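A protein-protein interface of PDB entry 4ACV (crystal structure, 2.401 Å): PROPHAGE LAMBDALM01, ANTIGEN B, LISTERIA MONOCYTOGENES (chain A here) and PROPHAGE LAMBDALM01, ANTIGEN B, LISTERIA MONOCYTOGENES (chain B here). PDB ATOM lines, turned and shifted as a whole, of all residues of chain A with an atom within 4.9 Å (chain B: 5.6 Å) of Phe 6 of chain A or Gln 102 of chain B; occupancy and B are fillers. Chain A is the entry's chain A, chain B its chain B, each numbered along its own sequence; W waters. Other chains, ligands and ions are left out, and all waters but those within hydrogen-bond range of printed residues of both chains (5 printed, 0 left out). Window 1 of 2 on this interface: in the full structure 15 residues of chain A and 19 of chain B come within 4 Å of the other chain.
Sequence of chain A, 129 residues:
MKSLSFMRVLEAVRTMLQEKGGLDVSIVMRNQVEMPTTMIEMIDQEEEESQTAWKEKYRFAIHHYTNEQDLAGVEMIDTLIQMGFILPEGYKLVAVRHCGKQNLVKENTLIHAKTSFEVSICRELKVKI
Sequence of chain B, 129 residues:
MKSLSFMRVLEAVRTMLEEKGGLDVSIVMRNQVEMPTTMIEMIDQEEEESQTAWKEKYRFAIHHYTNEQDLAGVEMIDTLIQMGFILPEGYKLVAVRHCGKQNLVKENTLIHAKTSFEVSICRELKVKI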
ATOM      1  N   LEU A   4       2.573   7.878  -3.808  1.00  0.00           N
ATOM      2  CA  LEU A   4       1.668   7.167  -4.705  1.00  0.00           C
ATOM      3  C   LEU A   4       2.311   5.891  -5.277  1.00  0.00           C
ATOM      4  O   LEU A   4       3.459   5.900  -5.739  1.00  0.00           O
ATOM      5  CB  LEU A   4       1.250   8.120  -5.828  1.00  0.00           C
ATOM      6  CG  LEU A   4      -0.138   8.070  -6.452  1.00  0.00           C
ATOM      7  CD1 LEU A   4      -1.199   8.054  -5.385  1.00  0.00           C
ATOM      8  CD2 LEU A   4      -0.337   9.261  -7.378  1.00  0.00           C
ATOM      9  N   SER A   5       1.575   4.788  -5.211  1.00  0.00           N
ATOM     10  CA  SER A   5       2.001   3.529  -5.810  1.00  0.00           C
ATOM     11  C   SER A   5       2.158   3.676  -7.333  1.00  0.00           C
ATOM     12  O   SER A   5       1.337   4.306  -7.990  1.00  0.00           O
ATOM     13  CB  SER A   5       0.978   2.437  -5.478  1.00  0.00           C
ATOM     14  OG  SER A   5       1.227   1.238  -6.192  1.00  0.00           O
ATOM     15  N   PHE A   6       3.212   3.100  -7.899  1.00  0.00           N
ATOM     16  CA  PHE A   6       3.426   3.179  -9.345  1.00  0.00           C
ATOM     17  C   PHE A   6       2.155   2.778 -10.106  1.00  0.00           C
ATOM     18  O   PHE A   6       1.800   3.369 -11.126  1.00  0.00           O
ATOM     19  CB  PHE A   6       4.605   2.295  -9.769  1.00  0.00           C
ATOM     20  CG  PHE A   6       4.289   0.822  -9.799  1.00  0.00           C
ATOM     21  CD1 PHE A   6       3.777   0.231 -10.954  1.00  0.00           C
ATOM     22  CD2 PHE A   6       4.517   0.021  -8.685  1.00  0.00           C
ATOM     23  CE1 PHE A   6       3.484  -1.125 -10.998  1.00  0.00           C
ATOM     24  CE2 PHE A   6       4.227  -1.339  -8.719  1.00  0.00           C
ATOM     25  CZ  PHE A   6       3.706  -1.912  -9.877  1.00  0.00           C
ATOM     26  N   MET A   7       1.463   1.776  -9.585  1.00  0.00           N
ATOM     27  CA  MET A   7       0.265   1.275 -10.234  1.00  0.00           C
ATOM     28  C   MET A   7      -0.826   2.343 -10.329  1.00  0.00           C
ATOM     29  O   MET A   7      -1.532   2.444 -11.327  1.00  0.00           O
ATOM     30  CB  MET A   7      -0.239   0.042  -9.497  1.00  0.00           C
ATOM     31  CG  MET A   7      -0.874  -0.961 -10.413  1.00  0.00           C
ATOM     32  SD  MET A   7      -1.254  -2.484  -9.563  1.00  0.00           S
ATOM     33  CE  MET A   7      -2.649  -3.032 -10.548  1.00  0.00           C
ATOM     34  N   ARG A   8      -0.954   3.145  -9.281  1.00  0.00           N
ATOM     35  CA  ARG A   8      -1.857   4.281  -9.309  1.00  0.00           C
ATOM     36  C   ARG A   8      -1.481   5.249 -10.445  1.00  0.00           C
ATOM     37  O   ARG A   8      -2.347   5.750 -11.168  1.00  0.00           O
ATOM     38  CB  ARG A   8      -1.824   4.993  -7.964  1.00  0.00           C
ATOM     39  CG  ARG A   8      -2.792   6.128  -7.873  1.00  0.00           C
ATOM     40  CD  ARG A   8      -4.187   5.692  -8.288  1.00  0.00           C
ATOM     41  NE  ARG A   8      -4.775   4.717  -7.370  1.00  0.00           N
ATOM     42  CZ  ARG A   8      -6.085   4.488  -7.261  1.00  0.00           C
ATOM     43  NH1 ARG A   8      -6.946   5.170  -8.007  1.00  0.00           N
ATOM     44  NH2 ARG A   8      -6.542   3.586  -6.401  1.00  0.00           N
ATOM     45  N   VAL A   9      -0.184   5.493 -10.610  1.00  0.00           N
ATOM     46  CA  VAL A   9       0.303   6.330 -11.701  1.00  0.00           C
ATOM     47  C   VAL A   9       0.002   5.717 -13.064  1.00  0.00           C
ATOM     48  O   VAL A   9      -0.458   6.414 -13.969  1.00  0.00           O
ATOM     49  CB  VAL A   9       1.819   6.581 -11.601  1.00  0.00           C
ATOM     50  CG1 VAL A   9       2.285   7.384 -12.814  1.00  0.00           C
ATOM     51  CG2 VAL A   9       2.153   7.290 -10.302  1.00  0.00           C
ATOM     52  N   LEU A  10       0.272   4.422 -13.210  1.00  0.00           N
ATOM     53  CA  LEU A  10      -0.102   3.695 -14.425  1.00  0.00           C
ATOM     54  C   LEU A  10      -1.586   3.899 -14.740  1.00  0.00           C
ATOM     55  O   LEU A  10      -1.951   4.222 -15.862  1.00  0.00           O
ATOM     56  CB  LEU A  10       0.199   2.198 -14.282  1.00  0.00           C
ATOM     57  CG  LEU A  10       1.656   1.728 -14.254  1.00  0.00           C
ATOM     58  CD1 LEU A  10       1.738   0.227 -13.944  1.00  0.00           C
ATOM     59  CD2 LEU A  10       2.393   2.060 -15.561  1.00  0.00           C
ATOM     60  N   MET A  42       5.932   0.188 -16.565  1.00  0.00           N
ATOM     61  CA  MET A  42       6.555   0.923 -15.479  1.00  0.00           C
ATOM     62  C   MET A  42       7.973   0.387 -15.349  1.00  0.00           C
ATOM     63  O   MET A  42       8.216  -0.804 -15.546  1.00  0.00           O
ATOM     64  CB  MET A  42       5.752   0.753 -14.178  1.00  0.00           C
ATOM     65  CG  MET A  42       6.245   1.582 -12.990  1.00  0.00           C
ATOM     66  SD  MET A  42       6.266   3.391 -13.199  1.00  0.00           S
ATOM     67  CE  MET A  42       4.547   3.742 -13.525  1.00  0.00           C
ATOM     68  N   ILE A  43       8.917   1.269 -15.055  1.00  0.00           N
ATOM     69  CA  ILE A  43      10.318   0.868 -14.984  1.00  0.00           C
ATOM     70  C   ILE A  43      10.910   1.052 -13.576  1.00  0.00           C
ATOM     71  O   ILE A  43      11.367   0.089 -12.956  1.00  0.00           O
ATOM     72  CB  ILE A  43      11.168   1.620 -16.033  1.00  0.00           C
ATOM     73  CG1 ILE A  43      10.666   1.318 -17.454  1.00  0.00           C
ATOM     74  CG2 ILE A  43      12.651   1.260 -15.895  1.00  0.00           C
ATOM     75  CD1 ILE A  43      11.260   2.237 -18.519  1.00  0.00           C
ATOM     76  N   ASP A  44      10.905   2.286 -13.077  1.00  0.00           N
ATOM     77  CA  ASP A  44      11.405   2.544 -11.729  1.00  0.00           C
ATOM     78  C   ASP A  44      10.890   3.846 -11.109  1.00  0.00           C
ATOM     79  O   ASP A  44      10.190   4.627 -11.752  1.00  0.00           O
ATOM     80  CB  ASP A  44      12.940   2.452 -11.663  1.00  0.00           C
ATOM     81  CG  ASP A  44      13.639   3.461 -12.565  1.00  0.00           C
ATOM     82  OD1 ASP A  44      13.024   4.480 -12.936  1.00  0.00           O
ATOM     83  OD2 ASP A  44      14.820   3.231 -12.892  1.00  0.00           O
ATOM     84  N   GLN A  45      11.232   4.057  -9.844  1.00  0.00           N
ATOM     85  CA  GLN A  45      10.713   5.175  -9.077  1.00  0.00           C
ATOM     86  C   GLN A  45      11.781   5.617  -8.094  1.00  0.00           C
ATOM     87  O   GLN A  45      12.517   4.796  -7.563  1.00  0.00           O
ATOM     88  CB  GLN A  45       9.448   4.745  -8.336  1.00  0.00           C
ATOM     89  CG  GLN A  45       8.682   5.856  -7.637  1.00  0.00           C
ATOM     90  CD  GLN A  45       7.450   5.321  -6.921  1.00  0.00           C
ATOM     91  OE1 GLN A  45       6.963   4.238  -7.238  1.00  0.00           O
ATOM     92  NE2 GLN A  45       6.943   6.080  -5.958  1.00  0.00           N
ATOM     93  N   TYR A  58       8.895   9.087 -11.476  1.00  0.00           N
ATOM     94  CA  TYR A  58       8.508   7.776 -11.974  1.00  0.00           C
ATOM     95  C   TYR A  58       8.969   7.697 -13.407  1.00  0.00           C
ATOM     96  O   TYR A  58       8.853   8.669 -14.154  1.00  0.00           O
ATOM     97  CB  TYR A  58       6.990   7.581 -11.937  1.00  0.00           C
ATOM     98  CG  TYR A  58       6.343   7.696 -10.571  1.00  0.00           C
ATOM     99  CD1 TYR A  58       6.339   8.902  -9.878  1.00  0.00           C
ATOM    100  CD2 TYR A  58       5.710   6.604  -9.984  1.00  0.00           C
ATOM    101  CE1 TYR A  58       5.747   9.009  -8.640  1.00  0.00           C
ATOM    102  CE2 TYR A  58       5.099   6.710  -8.741  1.00  0.00           C
ATOM    103  CZ  TYR A  58       5.124   7.913  -8.077  1.00  0.00           C
ATOM    104  OH  TYR A  58       4.517   8.025  -6.849  1.00  0.00           O
ATOM    105  N   VAL B  74      -2.372  -4.387  -4.098  1.00  0.00           N
ATOM    106  CA  VAL B  74      -1.046  -3.770  -4.227  1.00  0.00           C
ATOM    107  C   VAL B  74      -0.924  -2.498  -3.381  1.00  0.00           C
ATOM    108  O   VAL B  74       0.058  -2.303  -2.679  1.00  0.00           O
ATOM    109  CB  VAL B  74      -0.692  -3.472  -5.712  1.00  0.00           C
ATOM    110  CG1 VAL B  74       0.407  -2.445  -5.813  1.00  0.00           C
ATOM    111  CG2 VAL B  74      -0.275  -4.753  -6.414  1.00  0.00           C
ATOM    112  N   HIS B  98       9.870   4.510  -1.853  1.00  0.00           N
ATOM    113  CA  HIS B  98       9.930   3.777  -3.107  1.00  0.00           C
ATOM    114  C   HIS B  98      11.270   4.121  -3.709  1.00  0.00           C
ATOM    115  O   HIS B  98      11.670   5.279  -3.753  1.00  0.00           O
ATOM    116  CB  HIS B  98       8.834   4.192  -4.080  1.00  0.00           C
ATOM    117  CG  HIS B  98       7.453   3.852  -3.616  1.00  0.00           C
ATOM    118  ND1 HIS B  98       7.048   2.558  -3.376  1.00  0.00           N
ATOM    119  CD2 HIS B  98       6.377   4.635  -3.376  1.00  0.00           C
ATOM    120  CE1 HIS B  98       5.784   2.562  -2.993  1.00  0.00           C
ATOM    121  NE2 HIS B  98       5.357   3.809  -2.979  1.00  0.00           N
ATOM    122  N   CYS B  99      11.966   3.095  -4.161  1.00  0.00           N
ATOM    123  CA  CYS B  99      13.275   3.272  -4.708  1.00  0.00           C
ATOM    124  C   CYS B  99      13.601   2.050  -5.526  1.00  0.00           C
ATOM    125  O   CYS B  99      13.522   0.924  -5.035  1.00  0.00           O
ATOM    126  CB  CYS B  99      14.286   3.433  -3.573  1.00  0.00           C
ATOM    127  SG  CYS B  99      15.987   3.597  -4.141  1.00  0.00           S
ATOM    128  N   GLY B 100      13.973   2.280  -6.779  1.00  0.00           N
ATOM    129  CA  GLY B 100      14.346   1.200  -7.667  1.00  0.00           C
ATOM    130  C   GLY B 100      13.213   0.709  -8.557  1.00  0.00           C
ATOM    131  O   GLY B 100      12.261   1.435  -8.861  1.00  0.00           O
ATOM    132  N   LYS B 101      13.329  -0.549  -8.964  1.00  0.00           N
ATOM    133  CA  LYS B 101      12.447  -1.147  -9.958  1.00  0.00           C
ATOM    134  C   LYS B 101      11.009  -1.310  -9.498  1.00  0.00           C
ATOM    135  O   LYS B 101      10.725  -1.830  -8.415  1.00  0.00           O
ATOM    136  CB  LYS B 101      13.032  -2.468 -10.459  1.00  0.00           C
ATOM    137  CG  LYS B 101      14.095  -2.241 -11.535  1.00  0.00           C
ATOM    138  CD  LYS B 101      14.982  -3.453 -11.756  1.00  0.00           C
ATOM    139  N   GLN B 102      10.105  -0.817 -10.333  1.00  0.00           N
ATOM    140  CA  GLN B 102       8.682  -0.987 -10.110  1.00  0.00           C
ATOM    141  C   GLN B 102       8.102  -1.598 -11.375  1.00  0.00           C
ATOM    142  O   GLN B 102       8.246  -1.039 -12.455  1.00  0.00           O
ATOM    143  CB  GLN B 102       8.033   0.359  -9.812  1.00  0.00           C
ATOM    144  CG  GLN B 102       8.894   1.283  -8.948  1.00  0.00           C
ATOM    145  CD  GLN B 102       8.985   0.868  -7.480  1.00  0.00           C
ATOM    146  OE1 GLN B 102       8.036   0.339  -6.908  1.00  0.00           O
ATOM    147  NE2 GLN B 102      10.124   1.145  -6.863  1.00  0.00           N
ATOM    148  N   ASN B 103       7.472  -2.761 -11.251  1.00  0.00           N
ATOM    149  CA  ASN B 103       7.024  -3.490 -12.433  1.00  0.00           C
ATOM    150  C   ASN B 103       5.614  -4.035 -12.321  1.00  0.00           C
ATOM    151  O   ASN B 103       5.151  -4.390 -11.245  1.00  0.00           O
ATOM    152  CB  ASN B 103       7.966  -4.661 -12.742  1.00  0.00           C
ATOM    153  CG  ASN B 103       9.385  -4.212 -13.055  1.00  0.00           C
ATOM    154  OD1 ASN B 103       9.639  -3.041 -13.360  1.00  0.00           O
ATOM    155  ND2 ASN B 103      10.316  -5.146 -12.982  1.00  0.00           N
ATOM    156  N   LEU B 104       4.940  -4.101 -13.460  1.00  0.00           N
ATOM    157  CA  LEU B 104       3.665  -4.779 -13.554  1.00  0.00           C
ATOM    158  C   LEU B 104       3.735  -5.554 -14.853  1.00  0.00           C
ATOM    159  O   LEU B 104       3.667  -4.970 -15.940  1.00  0.00           O
ATOM    160  CB  LEU B 104       2.493  -3.784 -13.564  1.00  0.00           C
ATOM    161  CG  LEU B 104       1.110  -4.449 -13.471  1.00  0.00           C
ATOM    162  CD1 LEU B 104       1.014  -5.324 -12.221  1.00  0.00           C
ATOM    163  CD2 LEU B 104      -0.023  -3.427 -13.503  1.00  0.00           C
ATOM    164  N   ALA B 113       3.293  -8.169  -9.894  1.00  0.00           N
ATOM    165  CA  ALA B 113       3.562  -6.798  -9.468  1.00  0.00           C
ATOM    166  C   ALA B 113       4.754  -6.741  -8.522  1.00  0.00           C
ATOM    167  O   ALA B 113       4.836  -7.476  -7.544  1.00  0.00           O
ATOM    168  CB  ALA B 113       2.342  -6.177  -8.822  1.00  0.00           C
ATOM    169  N   LYS B 114       5.680  -5.849  -8.833  1.00  0.00           N
ATOM    170  CA  LYS B 114       6.906  -5.726  -8.089  1.00  0.00           C
ATOM    171  C   LYS B 114       7.093  -4.280  -7.639  1.00  0.00           C
ATOM    172  O   LYS B 114       7.126  -3.368  -8.459  1.00  0.00           O
ATOM    173  CB  LYS B 114       8.078  -6.169  -8.961  1.00  0.00           C
ATOM    174  CG  LYS B 114       9.403  -6.053  -8.278  1.00  0.00           C
ATOM    175  CD  LYS B 114      10.530  -6.433  -9.215  1.00  0.00           C
ATOM    176  CE  LYS B 114      11.869  -6.170  -8.548  1.00  0.00           C
ATOM    177  NZ  LYS B 114      12.990  -6.593  -9.404  1.00  0.00           N
ATOM    178  N   THR B 115       7.220  -4.087  -6.329  1.00  0.00           N
ATOM    179  CA  THR B 115       7.377  -2.761  -5.749  1.00  0.00           C
ATOM    180  C   THR B 115       8.648  -2.706  -4.911  1.00  0.00           C
ATOM    181  O   THR B 115       8.818  -3.486  -3.980  1.00  0.00           O
ATOM    182  CB  THR B 115       6.182  -2.418  -4.848  1.00  0.00           C
ATOM    183  OG1 THR B 115       4.970  -2.472  -5.615  1.00  0.00           O
ATOM    184  CG2 THR B 115       6.364  -1.035  -4.218  1.00  0.00           C
ATOM    185  N   SER B 116       9.534  -1.774  -5.233  1.00  0.00           N
ATOM    186  CA  SER B 116      10.826  -1.698  -4.567  1.00  0.00           C
ATOM    187  C   SER B 116      10.923  -0.560  -3.572  1.00  0.00           C
ATOM    188  O   SER B 116      10.577   0.590  -3.864  1.00  0.00           O
ATOM    189  CB  SER B 116      11.970  -1.634  -5.581  1.00  0.00           C
ATOM    190  OG  SER B 116      12.048  -2.855  -6.303  1.00  0.00           O
ATOM    191  N   PHE B 117      11.407  -0.912  -2.387  1.00  0.00           N
ATOM    192  CA  PHE B 117      11.553   0.022  -1.278  1.00  0.00           C
ATOM    193  C   PHE B 117      12.986   0.178  -0.811  1.00  0.00           C
ATOM    194  O   PHE B 117      13.827  -0.721  -0.955  1.00  0.00           O
ATOM    195  CB  PHE B 117      10.725  -0.451  -0.082  1.00  0.00           C
ATOM    196  CG  PHE B 117       9.241  -0.373  -0.299  1.00  0.00           C
ATOM    197  CD1 PHE B 117       8.560   0.826  -0.094  1.00  0.00           C
ATOM    198  CD2 PHE B 117       8.525  -1.492  -0.697  1.00  0.00           C
ATOM    199  CE1 PHE B 117       7.185   0.905  -0.286  1.00  0.00           C
ATOM    200  CE2 PHE B 117       7.150  -1.423  -0.889  1.00  0.00           C
ATOM    201  CZ  PHE B 117       6.480  -0.223  -0.682  1.00  0.00           C
HETATM  202  O   HOH W   1       3.222  -0.325  -5.064  1.00  0.00           O
HETATM  203  O   HOH W   2       6.454  -3.125 -15.833  1.00  0.00           O
HETATM  204  O   HOH W   3       5.619   2.166  -6.406  1.00  0.00           O
HETATM  205  O   HOH W   4      12.170  -2.571 -14.614  1.00  0.00           O
HETATM  206  O   HOH W   5       3.767  -2.027 -16.333  1.00  0.00           O
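N of Gln 45 of chain A lies within hydrogen-bond range of O of Gly 100 of chain B (3.0 Å).
O of Ile 43 of chain A is in hydrogen-bond range of N of Gln 102 of chain B (3.0 Å).
O of Met 42 of chain A sits close to OD1 of Asn 103 of chain B (3.4 Å).
The backbone carbonyl oxygen (O) of Met 42 of chain A sits close to the backbone carbonyl oxygen (O) of Gln 102 of chain B.
O of Ser 116 of chain B lies within hydrogen-bond range of N of Cys 99 of chain B (2.9 Å).
The backbone carbonyl oxygen (O) of Leu 4 of chain A is in hydrogen-bond range of the side-chain amide nitrogen (NE2) of Gln 45 of chain A, at 3.5 Å.
NE2 of Gln 45 of chain A is in hydrogen-bond range of OH of Tyr 58 of chain A.
The side-chain amide nitrogen (NE2) of Gln 102 of chain B sits at hydrogen-bond distance from the backbone carbonyl oxygen (O) of Ser 116 of chain B (3.1 Å).
The side-chain hydroxyl of Ser 116 of chain B sits at hydrogen-bond distance from the backbone carbonyl oxygen of Lys 101 of chain B (2.7 Å).
The side-chain hydroxyl (OH) of Tyr 58 of chain A sits at hydrogen-bond distance from the backbone carbonyl oxygen (O) of Leu 4 of chain A (2.6 Å).
CB of Gln 102 of chain B touches CD2 of Phe 6 of chain A (3.7 Å).
Phe 6 of chain A touches Asn 103 of chain B.
Phe 6 of chain A touches Lys 114 of chain B.
Phe 6 of chain A touches Thr 115 of chain B (CE2 to OG1, 3.4 Å).
CE of Met 7 of chain A touches CD2 of Leu 104 of chain B, at 3.97 Å.
O of Ile 43 of chain A touches CA of Lys 101 of chain B, 3.4 Å away.
OD1 of Asn 103 of chain B touches O of Ile 43 of chain A (3.6 Å).
Asp 44 of chain A touches Gln 102 of chain B (CA to N, 3.9 Å).
CA of Cys 99 of chain B touches O of Gln 45 of chain A (3.3 Å).
Gln 102 of chain B touches Gln 45 of chain A.
Phe 6 of chain A touches five residues of chain B.
Gln 102 of chain B touches just these residues of chain A: Phe 6 (3.7 Å), Met 42 (3.1 Å), Ile 43 (3.0 Å), Asp 44 (3.9 Å) and Gln 45 (3.6 Å).
Of the printed residues of chain B, Met 42 of chain A touches Gln 102 (3.1 Å) and Asn 103 (3.4 Å).
Printed residues of chain A within 4 Å of Cys 99 of chain B: Gln 45.
Printed residues of chain A within 4 Å of Lys 101 of chain B: Ile 43.
Printed residues of chain B within 4 Å of Ser 5 of chain A: Val 74.
Leu 10 of chain A touches none of the printed residues of chain B.
Tyr 58 of chain A touches none of the printed residues of chain B.
The nearest residue of chain B that does not touch Phe 6 of chain A is Ala 113 of chain B (4.6 Å).
The nearest printed residue of chain A that does not touch Thr 115 of chain B is Ser 5 of chain A (5.3 Å).
Among the printed residues, 19 pairs touch across the chains.
Among the printed residues, no Asp or Glu carboxylate lies within 4 Å of a Lys or Arg side-chain nitrogen of the other chain.
Water W3 lies within hydrogen-bond range of the side-chain amide oxygen of Gln 45 of chain A, the backbone NH of Phe 6 of chain A, the side-chain amide oxygen of Gln 102 of chain B and a ring nitrogen (ND1) of His 98 of chain B.
Water W1 bridges the side-chain hydroxyl (OG) of Ser 5 of chain A and the side-chain hydroxyl (OG1) of Thr 115 of chain B.
Water W4 lies within hydrogen-bond range of the side-chain amide oxygen of Asn 103 of chain B and the backbone carbonyl oxygen of Ile 43 of chain A.
Water W2 bridges O of Met 42 of chain A (2.9 Å) and N of Leu 104 of chain B (3.0 Å).
Water W5 bridges the backbone carbonyl oxygen of Leu 104 of chain B (3.0 Å) and the backbone NH of Met 42 of chain A (3.1 Å).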
